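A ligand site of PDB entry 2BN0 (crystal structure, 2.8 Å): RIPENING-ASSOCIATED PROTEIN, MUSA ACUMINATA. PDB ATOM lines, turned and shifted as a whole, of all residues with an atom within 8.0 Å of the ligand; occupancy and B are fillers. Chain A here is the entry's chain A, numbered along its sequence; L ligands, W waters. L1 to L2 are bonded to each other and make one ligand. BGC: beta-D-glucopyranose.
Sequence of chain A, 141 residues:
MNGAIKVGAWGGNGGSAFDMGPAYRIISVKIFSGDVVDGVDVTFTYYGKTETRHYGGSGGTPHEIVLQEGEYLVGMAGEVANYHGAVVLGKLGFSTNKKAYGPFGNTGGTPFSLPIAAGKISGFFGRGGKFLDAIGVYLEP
Merely in contact with the ligand: Gly 129, Gly 14 and Val 88. Hydrophobic or aromatic side chains that line the ligand: Val 88 and Phe 131. Of the 25 residues printed, 7 come within 4 Å of the ligand. Along chain A the residues within 4 Å of the ligand span positions 14 to 133. The nearest printed residue that does not touch the ligand is Ala 86 (4.5 Å).
The backbone NH (N) of Gly 57 is in hydrogen-bond range of the backbone carbonyl oxygen (O) of Gly 129, 3.4 Å away. The backbone NH (N) of Asp 133 lies within hydrogen-bond range of the backbone carbonyl oxygen (O) of Arg 127 (3.3 Å). OD1 of Asp 133 is in hydrogen-bond range of N of Gly 15, at 2.8 Å. O of Gly 14 lies within hydrogen-bond range of NE of Arg 127. The side-chain carboxylate (OD2) of Asp 133 lies within hydrogen-bond range of the backbone NH (N) of Gly 129 (3.3 Å). The backbone NH of Gly 12 is in hydrogen-bond range of the backbone carbonyl oxygen of Asp 133, 2.9 Å away. The backbone carbonyl oxygen of Gly 15 lies within hydrogen-bond range of the guanidinium group of Arg 127 (3.1 Å).
N of Gly 15 is in hydrogen-bond range of O3 of BGC L1 (3.1 Å). O6 of BGC L1 sits at hydrogen-bond distance from N of Lys 130 (2.8 Å). O6 of BGC L1 is in hydrogen-bond range of O of Phe 131 (3.3 Å). N of Phe 131 is in hydrogen-bond range of O6 of BGC L1 (2.6 Å). An oxygen (O4) of BGC L1 lies within hydrogen-bond range of the side-chain carboxylate of Asp 133, 2.9 Å away.
Water W1 bridges an oxygen (O2) of BGC L2 and the side-chain hydroxyl (OG) of Ser 16.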
ATOM      1  N   GLY A  12      21.325 -16.298 -18.519  1.00  0.00           N
ATOM      2  CA  GLY A  12      21.529 -15.269 -19.522  1.00  0.00           C
ATOM      3  C   GLY A  12      20.405 -15.220 -20.534  1.00  0.00           C
ATOM      4  O   GLY A  12      19.552 -16.105 -20.559  1.00  0.00           O
ATOM      5  N   ASN A  13      20.414 -14.193 -21.368  1.00  0.00           N
ATOM      6  CA  ASN A  13      19.383 -14.016 -22.388  1.00  0.00           C
ATOM      7  C   ASN A  13      19.659 -14.708 -23.721  1.00  0.00           C
ATOM      8  O   ASN A  13      18.832 -14.693 -24.624  1.00  0.00           O
ATOM      9  CB  ASN A  13      19.162 -12.523 -22.636  1.00  0.00           C
ATOM     10  CG  ASN A  13      18.694 -11.794 -21.399  1.00  0.00           C
ATOM     11  OD1 ASN A  13      17.634 -12.101 -20.841  1.00  0.00           O
ATOM     12  ND2 ASN A  13      19.485 -10.823 -20.949  1.00  0.00           N
ATOM     13  N   GLY A  14      20.843 -15.320 -23.843  1.00  0.00           N
ATOM     14  CA  GLY A  14      21.163 -16.002 -25.089  1.00  0.00           C
ATOM     15  C   GLY A  14      20.358 -17.280 -25.268  1.00  0.00           C
ATOM     16  O   GLY A  14      19.415 -17.536 -24.521  1.00  0.00           O
ATOM     17  N   GLY A  15      20.746 -18.075 -26.256  1.00  0.00           N
ATOM     18  CA  GLY A  15      20.068 -19.330 -26.528  1.00  0.00           C
ATOM     19  C   GLY A  15      18.641 -19.152 -27.015  1.00  0.00           C
ATOM     20  O   GLY A  15      18.216 -18.054 -27.357  1.00  0.00           O
ATOM     21  N   SER A  16      17.908 -20.261 -27.064  1.00  0.00           N
ATOM     22  CA  SER A  16      16.519 -20.246 -27.492  1.00  0.00           C
ATOM     23  C   SER A  16      15.627 -20.793 -26.397  1.00  0.00           C
ATOM     24  O   SER A  16      15.949 -21.788 -25.746  1.00  0.00           O
ATOM     25  CB  SER A  16      16.357 -21.087 -28.760  1.00  0.00           C
ATOM     26  OG  SER A  16      17.078 -20.516 -29.846  1.00  0.00           O
ATOM     27  N   VAL A  36      30.687 -25.898 -17.242  1.00  0.00           N
ATOM     28  CA  VAL A  36      29.400 -25.293 -16.953  1.00  0.00           C
ATOM     29  C   VAL A  36      28.310 -26.357 -17.056  1.00  0.00           C
ATOM     30  O   VAL A  36      28.598 -27.559 -17.125  1.00  0.00           O
ATOM     31  CB  VAL A  36      29.104 -24.182 -17.973  1.00  0.00           C
ATOM     32  CG1 VAL A  36      30.221 -23.176 -17.974  1.00  0.00           C
ATOM     33  CG2 VAL A  36      28.952 -24.780 -19.358  1.00  0.00           C
ATOM     34  N   VAL A  37      27.054 -25.915 -17.063  1.00  0.00           N
ATOM     35  CA  VAL A  37      25.925 -26.836 -17.198  1.00  0.00           C
ATOM     36  C   VAL A  37      25.595 -26.875 -18.681  1.00  0.00           C
ATOM     37  O   VAL A  37      25.307 -25.855 -19.303  1.00  0.00           O
ATOM     38  CB  VAL A  37      24.689 -26.356 -16.402  1.00  0.00           C
ATOM     39  CG1 VAL A  37      23.547 -27.339 -16.569  1.00  0.00           C
ATOM     40  CG2 VAL A  37      25.028 -26.215 -14.919  1.00  0.00           C
ATOM     41  N   ASP A  38      25.653 -28.069 -19.259  1.00  0.00           N
ATOM     42  CA  ASP A  38      25.381 -28.244 -20.672  1.00  0.00           C
ATOM     43  C   ASP A  38      23.890 -28.295 -20.980  1.00  0.00           C
ATOM     44  O   ASP A  38      23.385 -27.532 -21.798  1.00  0.00           O
ATOM     45  CB  ASP A  38      26.085 -29.507 -21.175  1.00  0.00           C
ATOM     46  CG  ASP A  38      27.592 -29.346 -21.209  1.00  0.00           C
ATOM     47  OD1 ASP A  38      28.092 -28.708 -22.150  1.00  0.00           O
ATOM     48  OD2 ASP A  38      28.255 -29.833 -20.267  1.00  0.00           O
ATOM     49  N   GLY A  56      18.940 -27.745 -23.350  1.00  0.00           N
ATOM     50  CA  GLY A  56      20.312 -27.273 -23.327  1.00  0.00           C
ATOM     51  C   GLY A  56      21.096 -27.980 -24.412  1.00  0.00           C
ATOM     52  O   GLY A  56      20.514 -28.498 -25.373  1.00  0.00           O
ATOM     53  N   GLY A  57      22.425 -28.001 -24.252  1.00  0.00           N
ATOM     54  CA  GLY A  57      23.280 -28.660 -25.222  1.00  0.00           C
ATOM     55  C   GLY A  57      23.453 -30.147 -24.988  1.00  0.00           C
ATOM     56  O   GLY A  57      23.012 -30.700 -23.969  1.00  0.00           O
ATOM     57  N   TYR A  83      30.697 -17.648 -19.710  1.00  0.00           N
ATOM     58  CA  TYR A  83      31.527 -18.705 -20.262  1.00  0.00           C
ATOM     59  C   TYR A  83      31.816 -18.448 -21.733  1.00  0.00           C
ATOM     60  O   TYR A  83      31.019 -18.761 -22.608  1.00  0.00           O
ATOM     61  CB  TYR A  83      30.815 -20.038 -20.115  1.00  0.00           C
ATOM     62  CG  TYR A  83      31.624 -21.253 -20.477  1.00  0.00           C
ATOM     63  CD1 TYR A  83      31.379 -21.961 -21.653  1.00  0.00           C
ATOM     64  CD2 TYR A  83      32.604 -21.741 -19.613  1.00  0.00           C
ATOM     65  CE1 TYR A  83      32.078 -23.131 -21.942  1.00  0.00           C
ATOM     66  CE2 TYR A  83      33.310 -22.899 -19.900  1.00  0.00           C
ATOM     67  CZ  TYR A  83      33.044 -23.596 -21.059  1.00  0.00           C
ATOM     68  OH  TYR A  83      33.719 -24.766 -21.309  1.00  0.00           O
ATOM     69  N   HIS A  84      32.981 -17.852 -21.983  1.00  0.00           N
ATOM     70  CA  HIS A  84      33.398 -17.530 -23.345  1.00  0.00           C
ATOM     71  C   HIS A  84      32.384 -16.634 -24.047  1.00  0.00           C
ATOM     72  O   HIS A  84      31.823 -17.003 -25.088  1.00  0.00           O
ATOM     73  CB  HIS A  84      33.646 -18.819 -24.144  1.00  0.00           C
ATOM     74  CG  HIS A  84      34.628 -19.754 -23.495  1.00  0.00           C
ATOM     75  ND1 HIS A  84      35.722 -19.308 -22.788  1.00  0.00           N
ATOM     76  CD2 HIS A  84      34.681 -21.107 -23.463  1.00  0.00           C
ATOM     77  CE1 HIS A  84      36.404 -20.341 -22.346  1.00  0.00           C
ATOM     78  NE2 HIS A  84      35.799 -21.447 -22.736  1.00  0.00           N
ATOM     79  N   GLY A  85      32.148 -15.460 -23.460  1.00  0.00           N
ATOM     80  CA  GLY A  85      31.217 -14.503 -24.021  1.00  0.00           C
ATOM     81  C   GLY A  85      29.766 -14.941 -24.010  1.00  0.00           C
ATOM     82  O   GLY A  85      28.974 -14.488 -24.836  1.00  0.00           O
ATOM     83  N   ALA A  86      29.412 -15.812 -23.086  1.00  0.00           N
ATOM     84  CA  ALA A  86      28.027 -16.284 -23.005  1.00  0.00           C
ATOM     85  C   ALA A  86      27.612 -16.514 -21.557  1.00  0.00           C
ATOM     86  O   ALA A  86      28.250 -17.276 -20.829  1.00  0.00           O
ATOM     87  CB  ALA A  86      27.872 -17.583 -23.814  1.00  0.00           C
ATOM     88  N   VAL A  87      26.552 -15.838 -21.140  1.00  0.00           N
ATOM     89  CA  VAL A  87      26.058 -15.975 -19.778  1.00  0.00           C
ATOM     90  C   VAL A  87      25.222 -17.252 -19.685  1.00  0.00           C
ATOM     91  O   VAL A  87      24.138 -17.329 -20.255  1.00  0.00           O
ATOM     92  CB  VAL A  87      25.182 -14.777 -19.370  1.00  0.00           C
ATOM     93  CG1 VAL A  87      24.775 -14.897 -17.908  1.00  0.00           C
ATOM     94  CG2 VAL A  87      25.943 -13.474 -19.611  1.00  0.00           C
ATOM     95  N   VAL A  88      25.739 -18.246 -18.975  1.00  0.00           N
ATOM     96  CA  VAL A  88      25.047 -19.512 -18.807  1.00  0.00           C
ATOM     97  C   VAL A  88      25.240 -20.004 -17.390  1.00  0.00           C
ATOM     98  O   VAL A  88      25.978 -19.406 -16.625  1.00  0.00           O
ATOM     99  CB  VAL A  88      25.600 -20.580 -19.781  1.00  0.00           C
ATOM    100  CG1 VAL A  88      25.556 -20.059 -21.214  1.00  0.00           C
ATOM    101  CG2 VAL A  88      27.016 -20.961 -19.394  1.00  0.00           C
ATOM    102  N   LEU A  89      24.581 -21.102 -17.037  1.00  0.00           N
ATOM    103  CA  LEU A  89      24.736 -21.658 -15.700  1.00  0.00           C
ATOM    104  C   LEU A  89      26.039 -22.438 -15.618  1.00  0.00           C
ATOM    105  O   LEU A  89      26.262 -23.377 -16.382  1.00  0.00           O
ATOM    106  CB  LEU A  89      23.569 -22.589 -15.355  1.00  0.00           C
ATOM    107  CG  LEU A  89      22.200 -21.979 -15.106  1.00  0.00           C
ATOM    108  CD1 LEU A  89      21.651 -21.359 -16.380  1.00  0.00           C
ATOM    109  CD2 LEU A  89      21.268 -23.050 -14.599  1.00  0.00           C
ATOM    110  N   ARG A 127      16.120 -21.172 -21.352  1.00  0.00           N
ATOM    111  CA  ARG A 127      16.730 -20.933 -22.642  1.00  0.00           C
ATOM    112  C   ARG A 127      17.913 -21.868 -22.813  1.00  0.00           C
ATOM    113  O   ARG A 127      18.710 -22.048 -21.902  1.00  0.00           O
ATOM    114  CB  ARG A 127      17.208 -19.492 -22.757  1.00  0.00           C
ATOM    115  CG  ARG A 127      16.148 -18.478 -22.388  1.00  0.00           C
ATOM    116  CD  ARG A 127      16.635 -17.069 -22.646  1.00  0.00           C
ATOM    117  NE  ARG A 127      16.730 -16.779 -24.073  1.00  0.00           N
ATOM    118  CZ  ARG A 127      15.685 -16.765 -24.892  1.00  0.00           C
ATOM    119  NH1 ARG A 127      14.476 -17.018 -24.436  1.00  0.00           N
ATOM    120  NH2 ARG A 127      15.864 -16.487 -26.187  1.00  0.00           N
ATOM    121  N   GLY A 128      18.011 -22.470 -23.995  1.00  0.00           N
ATOM    122  CA  GLY A 128      19.108 -23.388 -24.269  1.00  0.00           C
ATOM    123  C   GLY A 128      19.874 -23.023 -25.522  1.00  0.00           C
ATOM    124  O   GLY A 128      19.372 -22.333 -26.412  1.00  0.00           O
ATOM    125  N   GLY A 129      21.112 -23.503 -25.584  1.00  0.00           N
ATOM    126  CA  GLY A 129      21.968 -23.257 -26.734  1.00  0.00           C
ATOM    127  C   GLY A 129      23.005 -24.368 -26.760  1.00  0.00           C
ATOM    128  O   GLY A 129      22.658 -25.546 -26.653  1.00  0.00           O
ATOM    129  N   LYS A 130      24.273 -24.000 -26.896  1.00  0.00           N
ATOM    130  CA  LYS A 130      25.323 -25.010 -26.881  1.00  0.00           C
ATOM    131  C   LYS A 130      25.415 -25.464 -25.425  1.00  0.00           C
ATOM    132  O   LYS A 130      25.949 -26.530 -25.118  1.00  0.00           O
ATOM    133  CB  LYS A 130      26.656 -24.423 -27.342  1.00  0.00           C
ATOM    134  CG  LYS A 130      27.803 -25.420 -27.296  1.00  0.00           C
ATOM    135  CD  LYS A 130      29.046 -24.907 -28.005  1.00  0.00           C
ATOM    136  CE  LYS A 130      30.210 -25.860 -27.772  1.00  0.00           C
ATOM    137  NZ  LYS A 130      29.826 -27.276 -28.020  1.00  0.00           N
ATOM    138  N   PHE A 131      24.858 -24.628 -24.543  1.00  0.00           N
ATOM    139  CA  PHE A 131      24.833 -24.894 -23.107  1.00  0.00           C
ATOM    140  C   PHE A 131      23.497 -24.440 -22.513  1.00  0.00           C
ATOM    141  O   PHE A 131      22.591 -24.020 -23.223  1.00  0.00           O
ATOM    142  CB  PHE A 131      25.981 -24.171 -22.412  1.00  0.00           C
ATOM    143  CG  PHE A 131      27.327 -24.448 -23.014  1.00  0.00           C
ATOM    144  CD1 PHE A 131      27.944 -23.499 -23.835  1.00  0.00           C
ATOM    145  CD2 PHE A 131      27.970 -25.658 -22.775  1.00  0.00           C
ATOM    146  CE1 PHE A 131      29.183 -23.758 -24.413  1.00  0.00           C
ATOM    147  CE2 PHE A 131      29.209 -25.925 -23.348  1.00  0.00           C
ATOM    148  CZ  PHE A 131      29.819 -24.965 -24.169  1.00  0.00           C
ATOM    149  N   LEU A 132      23.389 -24.524 -21.190  1.00  0.00           N
ATOM    150  CA  LEU A 132      22.173 -24.123 -20.495  1.00  0.00           C
ATOM    151  C   LEU A 132      22.251 -22.649 -20.103  1.00  0.00           C
ATOM    152  O   LEU A 132      22.673 -22.307 -18.998  1.00  0.00           O
ATOM    153  CB  LEU A 132      21.990 -24.996 -19.246  1.00  0.00           C
ATOM    154  CG  LEU A 132      20.621 -24.968 -18.558  1.00  0.00           C
ATOM    155  CD1 LEU A 132      19.559 -25.440 -19.539  1.00  0.00           C
ATOM    156  CD2 LEU A 132      20.659 -25.845 -17.318  1.00  0.00           C
ATOM    157  N   ASP A 133      21.838 -21.768 -21.011  1.00  0.00           N
ATOM    158  CA  ASP A 133      21.875 -20.337 -20.766  1.00  0.00           C
ATOM    159  C   ASP A 133      21.097 -19.935 -19.506  1.00  0.00           C
ATOM    160  O   ASP A 133      21.597 -19.193 -18.665  1.00  0.00           O
ATOM    161  CB  ASP A 133      21.316 -19.558 -21.959  1.00  0.00           C
ATOM    162  CG  ASP A 133      21.934 -19.983 -23.272  1.00  0.00           C
ATOM    163  OD1 ASP A 133      22.246 -19.094 -24.103  1.00  0.00           O
ATOM    164  OD2 ASP A 133      22.090 -21.198 -23.503  1.00  0.00           O
ATOM    165  N   ALA A 134      19.872 -20.440 -19.390  1.00  0.00           N
ATOM    166  CA  ALA A 134      19.016 -20.122 -18.249  1.00  0.00           C
ATOM    167  C   ALA A 134      18.007 -21.226 -17.979  1.00  0.00           C
ATOM    168  O   ALA A 134      17.631 -21.982 -18.878  1.00  0.00           O
ATOM    169  CB  ALA A 134      18.297 -18.806 -18.510  1.00  0.00           C
HETATM  170  C2  BGC L   1      24.126 -20.220 -29.092  1.00  0.00           C
HETATM  171  C3  BGC L   1      23.891 -18.949 -28.283  1.00  0.00           C
HETATM  172  C4  BGC L   1      23.883 -19.212 -26.776  1.00  0.00           C
HETATM  173  C5  BGC L   1      25.012 -20.161 -26.330  1.00  0.00           C
HETATM  174  C6  BGC L   1      24.802 -20.686 -24.925  1.00  0.00           C
HETATM  175  C1  BGC L   1      25.321 -20.986 -28.532  1.00  0.00           C
HETATM  176  O1  BGC L   1      25.480 -22.171 -29.230  1.00  0.00           O
HETATM  177  O2  BGC L   1      24.359 -19.898 -30.448  1.00  0.00           O
HETATM  178  O3  BGC L   1      22.603 -18.431 -28.657  1.00  0.00           O
HETATM  179  O4  BGC L   1      24.017 -17.981 -26.094  1.00  0.00           O
HETATM  180  O5  BGC L   1      25.053 -21.319 -27.179  1.00  0.00           O
HETATM  181  O6  BGC L   1      24.672 -22.100 -24.918  1.00  0.00           O
HETATM  182  C2  BGC L   2      21.185 -17.139 -30.050  1.00  0.00           C
HETATM  183  C3  BGC L   2      21.032 -15.778 -30.722  1.00  0.00           C
HETATM  184  C4  BGC L   2      21.305 -14.683 -29.691  1.00  0.00           C
HETATM  185  C5  BGC L   2      22.704 -14.883 -29.121  1.00  0.00           C
HETATM  186  C6  BGC L   2      23.075 -13.856 -28.080  1.00  0.00           C
HETATM  187  C1  BGC L   2      22.566 -17.259 -29.396  1.00  0.00           C
HETATM  188  O2  BGC L   2      21.015 -18.172 -31.020  1.00  0.00           O
HETATM  189  O3  BGC L   2      19.721 -15.637 -31.246  1.00  0.00           O
HETATM  190  O4  BGC L   2      21.204 -13.410 -30.312  1.00  0.00           O
HETATM  191  O5  BGC L   2      22.790 -16.183 -28.487  1.00  0.00           O
HETATM  192  O6  BGC L   2      24.120 -14.337 -27.240  1.00  0.00           O
HETATM  193  O   HOH W   1      20.039 -20.553 -30.057  1.00  0.00           O
